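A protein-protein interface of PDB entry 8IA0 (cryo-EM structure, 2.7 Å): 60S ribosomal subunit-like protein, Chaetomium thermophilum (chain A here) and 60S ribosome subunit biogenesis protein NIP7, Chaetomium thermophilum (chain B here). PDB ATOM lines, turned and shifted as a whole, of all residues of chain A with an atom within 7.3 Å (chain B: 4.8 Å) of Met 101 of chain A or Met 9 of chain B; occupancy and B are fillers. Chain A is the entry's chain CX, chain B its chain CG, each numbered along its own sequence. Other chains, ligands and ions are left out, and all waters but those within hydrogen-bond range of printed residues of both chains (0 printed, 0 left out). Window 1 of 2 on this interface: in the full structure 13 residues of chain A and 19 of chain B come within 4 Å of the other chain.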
ATOM      1  N   VAL A  95       9.436 -20.201 -11.857  1.00  0.00           N
ATOM      2  CA  VAL A  95      10.739 -20.678 -11.417  1.00  0.00           C
ATOM      3  C   VAL A  95      11.645 -20.655 -12.640  1.00  0.00           C
ATOM      4  O   VAL A  95      11.421 -21.392 -13.608  1.00  0.00           O
ATOM      5  CB  VAL A  95      10.659 -22.079 -10.793  1.00  0.00           C
ATOM      6  CG1 VAL A  95      11.971 -22.831 -10.966  1.00  0.00           C
ATOM      7  CG2 VAL A  95      10.288 -21.981  -9.322  1.00  0.00           C
ATOM      8  N   ASP A  96      12.644 -19.777 -12.616  1.00  0.00           N
ATOM      9  CA  ASP A  96      13.592 -19.673 -13.715  1.00  0.00           C
ATOM     10  C   ASP A  96      15.037 -19.565 -13.265  1.00  0.00           C
ATOM     11  O   ASP A  96      15.931 -19.737 -14.098  1.00  0.00           O
ATOM     12  CB  ASP A  96      13.256 -18.466 -14.600  1.00  0.00           C
ATOM     13  CG  ASP A  96      13.506 -18.733 -16.071  1.00  0.00           C
ATOM     14  OD1 ASP A  96      14.258 -19.679 -16.386  1.00  0.00           O
ATOM     15  OD2 ASP A  96      12.954 -17.995 -16.913  1.00  0.00           O
ATOM     16  N   ASP A  97      15.303 -19.284 -11.995  1.00  0.00           N
ATOM     17  CA  ASP A  97      16.669 -19.208 -11.506  1.00  0.00           C
ATOM     18  C   ASP A  97      17.295 -20.593 -11.476  1.00  0.00           C
ATOM     19  O   ASP A  97      16.608 -21.597 -11.267  1.00  0.00           O
ATOM     20  CB  ASP A  97      16.705 -18.589 -10.109  1.00  0.00           C
ATOM     21  CG  ASP A  97      16.206 -17.158 -10.093  1.00  0.00           C
ATOM     22  OD1 ASP A  97      16.347 -16.465 -11.122  1.00  0.00           O
ATOM     23  OD2 ASP A  97      15.671 -16.726  -9.050  1.00  0.00           O
ATOM     24  N   ARG A  98      18.609 -20.645 -11.697  1.00  0.00           N
ATOM     25  CA  ARG A  98      19.332 -21.901 -11.546  1.00  0.00           C
ATOM     26  C   ARG A  98      19.250 -22.416 -10.117  1.00  0.00           C
ATOM     27  O   ARG A  98      19.179 -23.629  -9.894  1.00  0.00           O
ATOM     28  CB  ARG A  98      20.789 -21.716 -11.957  1.00  0.00           C
ATOM     29  CG  ARG A  98      21.428 -22.944 -12.557  1.00  0.00           C
ATOM     30  CD  ARG A  98      22.867 -22.663 -12.940  1.00  0.00           C
ATOM     31  NE  ARG A  98      23.784 -22.895 -11.831  1.00  0.00           N
ATOM     32  CZ  ARG A  98      24.140 -24.093 -11.389  1.00  0.00           C
ATOM     33  NH1 ARG A  98      23.678 -25.201 -11.945  1.00  0.00           N
ATOM     34  NH2 ARG A  98      24.984 -24.182 -10.365  1.00  0.00           N
ATOM     35  N   GLU A  99      19.267 -21.509  -9.143  1.00  0.00           N
ATOM     36  CA  GLU A  99      19.190 -21.906  -7.742  1.00  0.00           C
ATOM     37  C   GLU A  99      17.824 -22.491  -7.406  1.00  0.00           C
ATOM     38  O   GLU A  99      17.727 -23.492  -6.687  1.00  0.00           O
ATOM     39  CB  GLU A  99      19.503 -20.703  -6.855  1.00  0.00           C
ATOM     40  CG  GLU A  99      20.895 -20.134  -7.076  1.00  0.00           C
ATOM     41  CD  GLU A  99      20.940 -19.120  -8.204  1.00  0.00           C
ATOM     42  OE1 GLU A  99      20.076 -18.221  -8.236  1.00  0.00           O
ATOM     43  OE2 GLU A  99      21.842 -19.225  -9.061  1.00  0.00           O
ATOM     44  N   SER A 100      16.753 -21.880  -7.916  1.00  0.00           N
ATOM     45  CA  SER A 100      15.415 -22.400  -7.653  1.00  0.00           C
ATOM     46  C   SER A 100      15.210 -23.756  -8.315  1.00  0.00           C
ATOM     47  O   SER A 100      14.529 -24.629  -7.766  1.00  0.00           O
ATOM     48  CB  SER A 100      14.360 -21.406  -8.131  1.00  0.00           C
ATOM     49  OG  SER A 100      14.795 -20.073  -7.938  1.00  0.00           O
ATOM     50  N   MET A 101      15.785 -23.949  -9.501  1.00  0.00           N
ATOM     51  CA  MET A 101      15.672 -25.236 -10.175  1.00  0.00           C
ATOM     52  C   MET A 101      16.473 -26.312  -9.450  1.00  0.00           C
ATOM     53  O   MET A 101      16.095 -27.488  -9.455  1.00  0.00           O
ATOM     54  CB  MET A 101      16.131 -25.106 -11.626  1.00  0.00           C
ATOM     55  CG  MET A 101      15.212 -24.262 -12.491  1.00  0.00           C
ATOM     56  SD  MET A 101      15.376 -24.626 -14.246  1.00  0.00           S
ATOM     57  CE  MET A 101      16.726 -23.538 -14.684  1.00  0.00           C
ATOM     58  N   ASN A 102      17.589 -25.926  -8.826  1.00  0.00           N
ATOM     59  CA  ASN A 102      18.419 -26.896  -8.120  1.00  0.00           C
ATOM     60  C   ASN A 102      17.687 -27.501  -6.930  1.00  0.00           C
ATOM     61  O   ASN A 102      17.823 -28.698  -6.652  1.00  0.00           O
ATOM     62  CB  ASN A 102      19.722 -26.242  -7.669  1.00  0.00           C
ATOM     63  CG  ASN A 102      20.874 -26.569  -8.580  1.00  0.00           C
ATOM     64  OD1 ASN A 102      21.124 -27.730  -8.897  1.00  0.00           O
ATOM     65  ND2 ASN A 102      21.593 -25.541  -9.009  1.00  0.00           N
ATOM     66  N   THR A 103      16.920 -26.688  -6.203  1.00  0.00           N
ATOM     67  CA  THR A 103      16.185 -27.200  -5.051  1.00  0.00           C
ATOM     68  C   THR A 103      15.149 -28.231  -5.478  1.00  0.00           C
ATOM     69  O   THR A 103      15.035 -29.301  -4.869  1.00  0.00           O
ATOM     70  CB  THR A 103      15.517 -26.052  -4.297  1.00  0.00           C
ATOM     71  OG1 THR A 103      16.475 -25.017  -4.046  1.00  0.00           O
ATOM     72  CG2 THR A 103      14.954 -26.544  -2.977  1.00  0.00           C
ATOM     73  N   ILE A 104      14.387 -27.929  -6.529  1.00  0.00           N
ATOM     74  CA  ILE A 104      13.390 -28.875  -7.020  1.00  0.00           C
ATOM     75  C   ILE A 104      14.068 -30.136  -7.534  1.00  0.00           C
ATOM     76  O   ILE A 104      13.582 -31.254  -7.325  1.00  0.00           O
ATOM     77  CB  ILE A 104      12.518 -28.216  -8.104  1.00  0.00           C
ATOM     78  CG1 ILE A 104      11.653 -27.117  -7.490  1.00  0.00           C
ATOM     79  CG2 ILE A 104      11.648 -29.248  -8.796  1.00  0.00           C
ATOM     80  CD1 ILE A 104      11.429 -25.944  -8.406  1.00  0.00           C
ATOM     81  N   LEU A 105      15.210 -29.976  -8.202  1.00  0.00           N
ATOM     82  CA  LEU A 105      15.905 -31.120  -8.777  1.00  0.00           C
ATOM     83  C   LEU A 105      16.430 -32.058  -7.696  1.00  0.00           C
ATOM     84  O   LEU A 105      16.407 -33.283  -7.866  1.00  0.00           O
ATOM     85  CB  LEU A 105      17.041 -30.636  -9.671  1.00  0.00           C
ATOM     86  CG  LEU A 105      17.773 -31.761 -10.383  1.00  0.00           C
ATOM     87  CD1 LEU A 105      16.779 -32.462 -11.279  1.00  0.00           C
ATOM     88  CD2 LEU A 105      18.939 -31.221 -11.183  1.00  0.00           C
ATOM     89  N   ALA A 106      16.918 -31.505  -6.583  1.00  0.00           N
ATOM     90  CA  ALA A 106      17.464 -32.341  -5.517  1.00  0.00           C
ATOM     91  C   ALA A 106      16.393 -33.231  -4.901  1.00  0.00           C
ATOM     92  O   ALA A 106      16.647 -34.405  -4.608  1.00  0.00           O
ATOM     93  CB  ALA A 106      18.118 -31.468  -4.449  1.00  0.00           C
ATOM     94  N   MET A 107      15.192 -32.690  -4.686  1.00  0.00           N
ATOM     95  CA  MET A 107      14.098 -33.498  -4.157  1.00  0.00           C
ATOM     96  C   MET A 107      13.726 -34.620  -5.116  1.00  0.00           C
ATOM     97  O   MET A 107      13.470 -35.752  -4.690  1.00  0.00           O
ATOM     98  CB  MET A 107      12.878 -32.623  -3.878  1.00  0.00           C
ATOM     99  CG  MET A 107      13.186 -31.267  -3.282  1.00  0.00           C
ATOM    100  SD  MET A 107      12.716 -31.165  -1.551  1.00  0.00           S
ATOM    101  CE  MET A 107      11.067 -30.484  -1.718  1.00  0.00           C
ATOM    102  N   VAL A 108      13.672 -34.317  -6.413  1.00  0.00           N
ATOM    103  CA  VAL A 108      13.298 -35.320  -7.406  1.00  0.00           C
ATOM    104  C   VAL A 108      14.315 -36.452  -7.424  1.00  0.00           C
ATOM    105  O   VAL A 108      13.958 -37.635  -7.466  1.00  0.00           O
ATOM    106  CB  VAL A 108      13.153 -34.668  -8.792  1.00  0.00           C
ATOM    107  CG1 VAL A 108      13.047 -35.726  -9.874  1.00  0.00           C
ATOM    108  CG2 VAL A 108      11.950 -33.745  -8.821  1.00  0.00           C
ATOM    109  N   GLU A 136      19.182 -21.000  -2.311  1.00  0.00           N
ATOM    110  CA  GLU A 136      17.996 -20.373  -2.885  1.00  0.00           C
ATOM    111  C   GLU A 136      17.460 -19.272  -1.982  1.00  0.00           C
ATOM    112  O   GLU A 136      17.083 -18.196  -2.461  1.00  0.00           O
ATOM    113  CB  GLU A 136      16.918 -21.424  -3.139  1.00  0.00           C
ATOM    114  CG  GLU A 136      15.659 -20.865  -3.768  1.00  0.00           C
ATOM    115  CD  GLU A 136      14.565 -21.902  -3.900  1.00  0.00           C
ATOM    116  OE1 GLU A 136      14.771 -23.045  -3.442  1.00  0.00           O
ATOM    117  OE2 GLU A 136      13.498 -21.576  -4.463  1.00  0.00           O
ATOM    118  N   LYS A 140      17.286 -15.351  -3.079  1.00  0.00           N
ATOM    119  CA  LYS A 140      16.047 -14.582  -3.081  1.00  0.00           C
ATOM    120  C   LYS A 140      16.121 -13.417  -2.105  1.00  0.00           C
ATOM    121  O   LYS A 140      15.508 -12.367  -2.333  1.00  0.00           O
ATOM    122  CB  LYS A 140      14.865 -15.491  -2.753  1.00  0.00           C
ATOM    123  CG  LYS A 140      14.421 -16.364  -3.915  1.00  0.00           C
ATOM    124  CD  LYS A 140      13.167 -17.146  -3.572  1.00  0.00           C
ATOM    125  CE  LYS A 140      12.580 -17.812  -4.803  1.00  0.00           C
ATOM    126  NZ  LYS A 140      13.480 -18.864  -5.351  1.00  0.00           N
ATOM    127  N   LEU B   4       8.206 -21.912 -16.540  1.00  0.00           N
ATOM    128  CA  LEU B   4       7.400 -22.865 -15.792  1.00  0.00           C
ATOM    129  C   LEU B   4       7.199 -22.403 -14.354  1.00  0.00           C
ATOM    130  O   LEU B   4       8.042 -21.716 -13.771  1.00  0.00           O
ATOM    131  CB  LEU B   4       8.058 -24.242 -15.801  1.00  0.00           C
ATOM    132  CG  LEU B   4       8.349 -24.866 -17.165  1.00  0.00           C
ATOM    133  CD1 LEU B   4       8.708 -26.331 -17.009  1.00  0.00           C
ATOM    134  CD2 LEU B   4       7.166 -24.700 -18.089  1.00  0.00           C
ATOM    135  N   THR B   5       6.063 -22.788 -13.784  1.00  0.00           N
ATOM    136  CA  THR B   5       5.814 -22.615 -12.365  1.00  0.00           C
ATOM    137  C   THR B   5       6.488 -23.754 -11.603  1.00  0.00           C
ATOM    138  O   THR B   5       7.036 -24.687 -12.193  1.00  0.00           O
ATOM    139  CB  THR B   5       4.314 -22.558 -12.084  1.00  0.00           C
ATOM    140  OG1 THR B   5       3.700 -23.778 -12.512  1.00  0.00           O
ATOM    141  CG2 THR B   5       3.679 -21.394 -12.826  1.00  0.00           C
ATOM    142  N   ASP B   6       6.460 -23.682 -10.271  1.00  0.00           N
ATOM    143  CA  ASP B   6       7.185 -24.677  -9.487  1.00  0.00           C
ATOM    144  C   ASP B   6       6.482 -26.031  -9.504  1.00  0.00           C
ATOM    145  O   ASP B   6       7.134 -27.071  -9.357  1.00  0.00           O
ATOM    146  CB  ASP B   6       7.409 -24.178  -8.057  1.00  0.00           C
ATOM    147  CG  ASP B   6       6.220 -24.409  -7.156  1.00  0.00           C
ATOM    148  OD1 ASP B   6       5.127 -23.905  -7.476  1.00  0.00           O
ATOM    149  OD2 ASP B   6       6.378 -25.095  -6.125  1.00  0.00           O
ATOM    150  N   GLN B   7       5.156 -26.050  -9.675  1.00  0.00           N
ATOM    151  CA  GLN B   7       4.482 -27.335  -9.848  1.00  0.00           C
ATOM    152  C   GLN B   7       4.867 -27.978 -11.174  1.00  0.00           C
ATOM    153  O   GLN B   7       5.120 -29.186 -11.236  1.00  0.00           O
ATOM    154  CB  GLN B   7       2.958 -27.191  -9.776  1.00  0.00           C
ATOM    155  CG  GLN B   7       2.360 -25.992 -10.498  1.00  0.00           C
ATOM    156  CD  GLN B   7       2.284 -24.753  -9.633  1.00  0.00           C
ATOM    157  OE1 GLN B   7       2.892 -24.688  -8.570  1.00  0.00           O
ATOM    158  NE2 GLN B   7       1.527 -23.761 -10.086  1.00  0.00           N
ATOM    159  N   GLU B   8       4.914 -27.182 -12.244  1.00  0.00           N
ATOM    160  CA  GLU B   8       5.173 -27.729 -13.571  1.00  0.00           C
ATOM    161  C   GLU B   8       6.615 -28.195 -13.711  1.00  0.00           C
ATOM    162  O   GLU B   8       6.884 -29.221 -14.347  1.00  0.00           O
ATOM    163  CB  GLU B   8       4.832 -26.684 -14.630  1.00  0.00           C
ATOM    164  CG  GLU B   8       3.397 -26.200 -14.556  1.00  0.00           C
ATOM    165  CD  GLU B   8       3.019 -25.303 -15.714  1.00  0.00           C
ATOM    166  OE1 GLU B   8       3.752 -24.327 -15.974  1.00  0.00           O
ATOM    167  OE2 GLU B   8       1.986 -25.572 -16.362  1.00  0.00           O
ATOM    168  N   MET B   9       7.559 -27.453 -13.129  1.00  0.00           N
ATOM    169  CA  MET B   9       8.960 -27.855 -13.196  1.00  0.00           C
ATOM    170  C   MET B   9       9.182 -29.186 -12.491  1.00  0.00           C
ATOM    171  O   MET B   9       9.980 -30.013 -12.945  1.00  0.00           O
ATOM    172  CB  MET B   9       9.847 -26.769 -12.592  1.00  0.00           C
ATOM    173  CG  MET B   9      11.323 -26.943 -12.887  1.00  0.00           C
ATOM    174  SD  MET B   9      11.709 -26.783 -14.638  1.00  0.00           S
ATOM    175  CE  MET B   9      11.566 -25.012 -14.855  1.00  0.00           C
ATOM    176  N   LYS B  10       8.486 -29.408 -11.376  1.00  0.00           N
ATOM    177  CA  LYS B  10       8.593 -30.684 -10.676  1.00  0.00           C
ATOM    178  C   LYS B  10       8.070 -31.829 -11.533  1.00  0.00           C
ATOM    179  O   LYS B  10       8.669 -32.909 -11.572  1.00  0.00           O
ATOM    180  CB  LYS B  10       7.835 -30.614  -9.352  1.00  0.00           C
ATOM    181  CG  LYS B  10       8.012 -31.832  -8.469  1.00  0.00           C
ATOM    182  CD  LYS B  10       6.820 -32.022  -7.553  1.00  0.00           C
ATOM    183  CE  LYS B  10       7.138 -32.991  -6.430  1.00  0.00           C
ATOM    184  NZ  LYS B  10       8.310 -32.547  -5.627  1.00  0.00           N
ATOM    185  N   ILE B  11       6.947 -31.615 -12.220  1.00  0.00           N
ATOM    186  CA  ILE B  11       6.368 -32.660 -13.062  1.00  0.00           C
ATOM    187  C   ILE B  11       7.294 -32.976 -14.230  1.00  0.00           C
ATOM    188  O   ILE B  11       7.497 -34.143 -14.586  1.00  0.00           O
ATOM    189  CB  ILE B  11       4.970 -32.239 -13.548  1.00  0.00           C
ATOM    190  CG1 ILE B  11       4.043 -32.012 -12.357  1.00  0.00           C
ATOM    191  CG2 ILE B  11       4.388 -33.288 -14.475  1.00  0.00           C
ATOM    192  CD1 ILE B  11       2.688 -31.464 -12.736  1.00  0.00           C
ATOM    193  N   VAL B  12       7.863 -31.940 -14.848  1.00  0.00           N
ATOM    194  CA  VAL B  12       8.726 -32.143 -16.008  1.00  0.00           C
ATOM    195  C   VAL B  12       9.982 -32.911 -15.613  1.00  0.00           C
ATOM    196  O   VAL B  12      10.405 -33.843 -16.306  1.00  0.00           O
ATOM    197  CB  VAL B  12       9.068 -30.792 -16.661  1.00  0.00           C
ATOM    198  CG1 VAL B  12      10.170 -30.959 -17.688  1.00  0.00           C
ATOM    199  CG2 VAL B  12       7.833 -30.192 -17.298  1.00  0.00           C
ATOM    200  N   LEU B  13      10.592 -32.537 -14.486  1.00  0.00           N
ATOM    201  CA  LEU B  13      11.831 -33.187 -14.074  1.00  0.00           C
ATOM    202  C   LEU B  13      11.587 -34.600 -13.563  1.00  0.00           C
ATOM    203  O   LEU B  13      12.469 -35.458 -13.682  1.00  0.00           O
ATOM    204  CB  LEU B  13      12.535 -32.350 -13.009  1.00  0.00           C
ATOM    205  CG  LEU B  13      13.054 -30.985 -13.464  1.00  0.00           C
ATOM    206  CD1 LEU B  13      13.612 -30.200 -12.289  1.00  0.00           C
ATOM    207  CD2 LEU B  13      14.105 -31.145 -14.543  1.00  0.00           C
ATOM    208  N   ILE B  27      21.068 -28.147 -16.545  1.00  0.00           N
ATOM    209  CA  ILE B  27      20.900 -26.740 -16.211  1.00  0.00           C
ATOM    210  C   ILE B  27      22.190 -26.109 -15.700  1.00  0.00           C
ATOM    211  O   ILE B  27      22.168 -24.976 -15.211  1.00  0.00           O
ATOM    212  CB  ILE B  27      19.760 -26.551 -15.201  1.00  0.00           C
ATOM    213  CG1 ILE B  27      20.174 -27.083 -13.829  1.00  0.00           C
ATOM    214  CG2 ILE B  27      18.502 -27.249 -15.685  1.00  0.00           C
ATOM    215  CD1 ILE B  27      19.162 -26.819 -12.748  1.00  0.00           C
ATOM    216  N   ARG B  35      23.101 -20.498 -19.946  1.00  0.00           N
ATOM    217  CA  ARG B  35      22.521 -21.716 -19.402  1.00  0.00           C
ATOM    218  C   ARG B  35      21.255 -22.068 -20.167  1.00  0.00           C
ATOM    219  O   ARG B  35      20.669 -21.234 -20.861  1.00  0.00           O
ATOM    220  CB  ARG B  35      22.210 -21.575 -17.909  1.00  0.00           C
ATOM    221  CG  ARG B  35      21.149 -20.547 -17.599  1.00  0.00           C
ATOM    222  CD  ARG B  35      21.372 -19.919 -16.241  1.00  0.00           C
ATOM    223  NE  ARG B  35      20.394 -18.878 -15.944  1.00  0.00           N
ATOM    224  CZ  ARG B  35      19.098 -19.087 -15.760  1.00  0.00           C
ATOM    225  NH1 ARG B  35      18.579 -20.303 -15.796  1.00  0.00           N
ATOM    226  NH2 ARG B  35      18.301 -18.050 -15.524  1.00  0.00           N
ATOM    227  N   TYR B  36      20.843 -23.323 -20.026  1.00  0.00           N
ATOM    228  CA  TYR B  36      19.613 -23.813 -20.624  1.00  0.00           C
ATOM    229  C   TYR B  36      18.449 -23.614 -19.664  1.00  0.00           C
ATOM    230  O   TYR B  36      18.596 -23.770 -18.450  1.00  0.00           O
ATOM    231  CB  TYR B  36      19.748 -25.291 -20.982  1.00  0.00           C
ATOM    232  CG  TYR B  36      20.416 -25.549 -22.308  1.00  0.00           C
ATOM    233  CD1 TYR B  36      19.683 -25.577 -23.483  1.00  0.00           C
ATOM    234  CD2 TYR B  36      21.783 -25.765 -22.387  1.00  0.00           C
ATOM    235  CE1 TYR B  36      20.291 -25.816 -24.697  1.00  0.00           C
ATOM    236  CE2 TYR B  36      22.401 -26.002 -23.597  1.00  0.00           C
ATOM    237  CZ  TYR B  36      21.651 -26.026 -24.748  1.00  0.00           C
ATOM    238  OH  TYR B  36      22.263 -26.264 -25.955  1.00  0.00           O
ATOM    239  N   VAL B  37      17.287 -23.270 -20.217  1.00  0.00           N
ATOM    240  CA  VAL B  37      16.089 -23.007 -19.438  1.00  0.00           C
ATOM    241  C   VAL B  37      14.938 -23.823 -20.013  1.00  0.00           C
ATOM    242  O   VAL B  37      15.066 -24.483 -21.044  1.00  0.00           O
ATOM    243  CB  VAL B  37      15.729 -21.510 -19.414  1.00  0.00           C
ATOM    244  CG1 VAL B  37      16.680 -20.753 -18.508  1.00  0.00           C
ATOM    245  CG2 VAL B  37      15.760 -20.939 -20.819  1.00  0.00           C
ATOM    246  N   PHE B  38      13.803 -23.771 -19.325  1.00  0.00           N
ATOM    247  CA  PHE B  38      12.576 -24.425 -19.758  1.00  0.00           C
ATOM    248  C   PHE B  38      11.532 -23.359 -20.048  1.00  0.00           C
ATOM    249  O   PHE B  38      11.377 -22.411 -19.272  1.00  0.00           O
ATOM    250  CB  PHE B  38      12.053 -25.395 -18.695  1.00  0.00           C
ATOM    251  CG  PHE B  38      12.909 -26.612 -18.505  1.00  0.00           C
ATOM    252  CD1 PHE B  38      14.057 -26.554 -17.741  1.00  0.00           C
ATOM    253  CD2 PHE B  38      12.556 -27.816 -19.081  1.00  0.00           C
ATOM    254  CE1 PHE B  38      14.841 -27.670 -17.564  1.00  0.00           C
ATOM    255  CE2 PHE B  38      13.336 -28.934 -18.906  1.00  0.00           C
ATOM    256  CZ  PHE B  38      14.477 -28.863 -18.147  1.00  0.00           C
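Of the 15 printed residues of chain B, 8 touch a printed residue of chain A. Of the 16 printed residues of chain A, 6 touch a printed residue of chain B. Printed residues of chain A that touch a printed residue of chain B: Val 95, Asp 96, Arg 98, Met 101, Ile 104 and Val 108. Hydrophobic or aromatic side chains of chain A that line the printed part of chain B: Val 95, Met 101, Ile 104 and Val 108.
The side-chain amide nitrogen (ND2) of Asn 102 of chain A lies within hydrogen-bond range of the backbone carbonyl oxygen (O) of Arg 98 of chain A, at 3.2 Å. The side-chain amide oxygen of Gln 7 of chain B sits close to the side-chain carboxylate of Asp 6 of chain B, at 2.6 Å.
Asp 97 of chain A touches none of the printed residues of chain B. Of the printed residues of chain B, Val 108 of chain A touches Leu 13. Of the printed residues of chain A, Asp 6 of chain B touches Val 95. Met 9 of chain B touches two residues of chain A. Of the printed residues of chain A, Lys 10 of chain B touches Ile 104 (3.9 Å). Printed residues of chain A within 4 Å of Arg 35 of chain B: Asp 96 (3.2 Å) and Met 101 (3.9 Å).
The backbone carbonyl oxygen (O) of Leu 4 of chain B is in hydrogen-bond range of the backbone NH (N) of Val 95 of chain A, at 2.8 Å. O of Asp 96 of chain A lies within hydrogen-bond range of NH1 of Arg 35 of chain B (3.2 Å).
Among the printed residues, merely in contact across the chains: Val 95 of chain A with Asp 6 of chain B (3.8 Å), Val 95 of chain A with Met 9 of chain B (3.8 Å), Asp 96 of chain A with Val 37 of chain B (3.4 Å), Arg 98 of chain A with Ile 27 of chain B (3.3 Å), Met 101 of chain A with Met 9 of chain B (3.9 Å), Met 101 of chain A with Ile 27 of chain B (3.7 Å), Met 101 of chain A with Arg 35 of chain B (3.9 Å), Ile 104 of chain A with Lys 10 of chain B (3.9 Å) and Val 108 of chain A with Leu 13 of chain B (3.9 Å).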
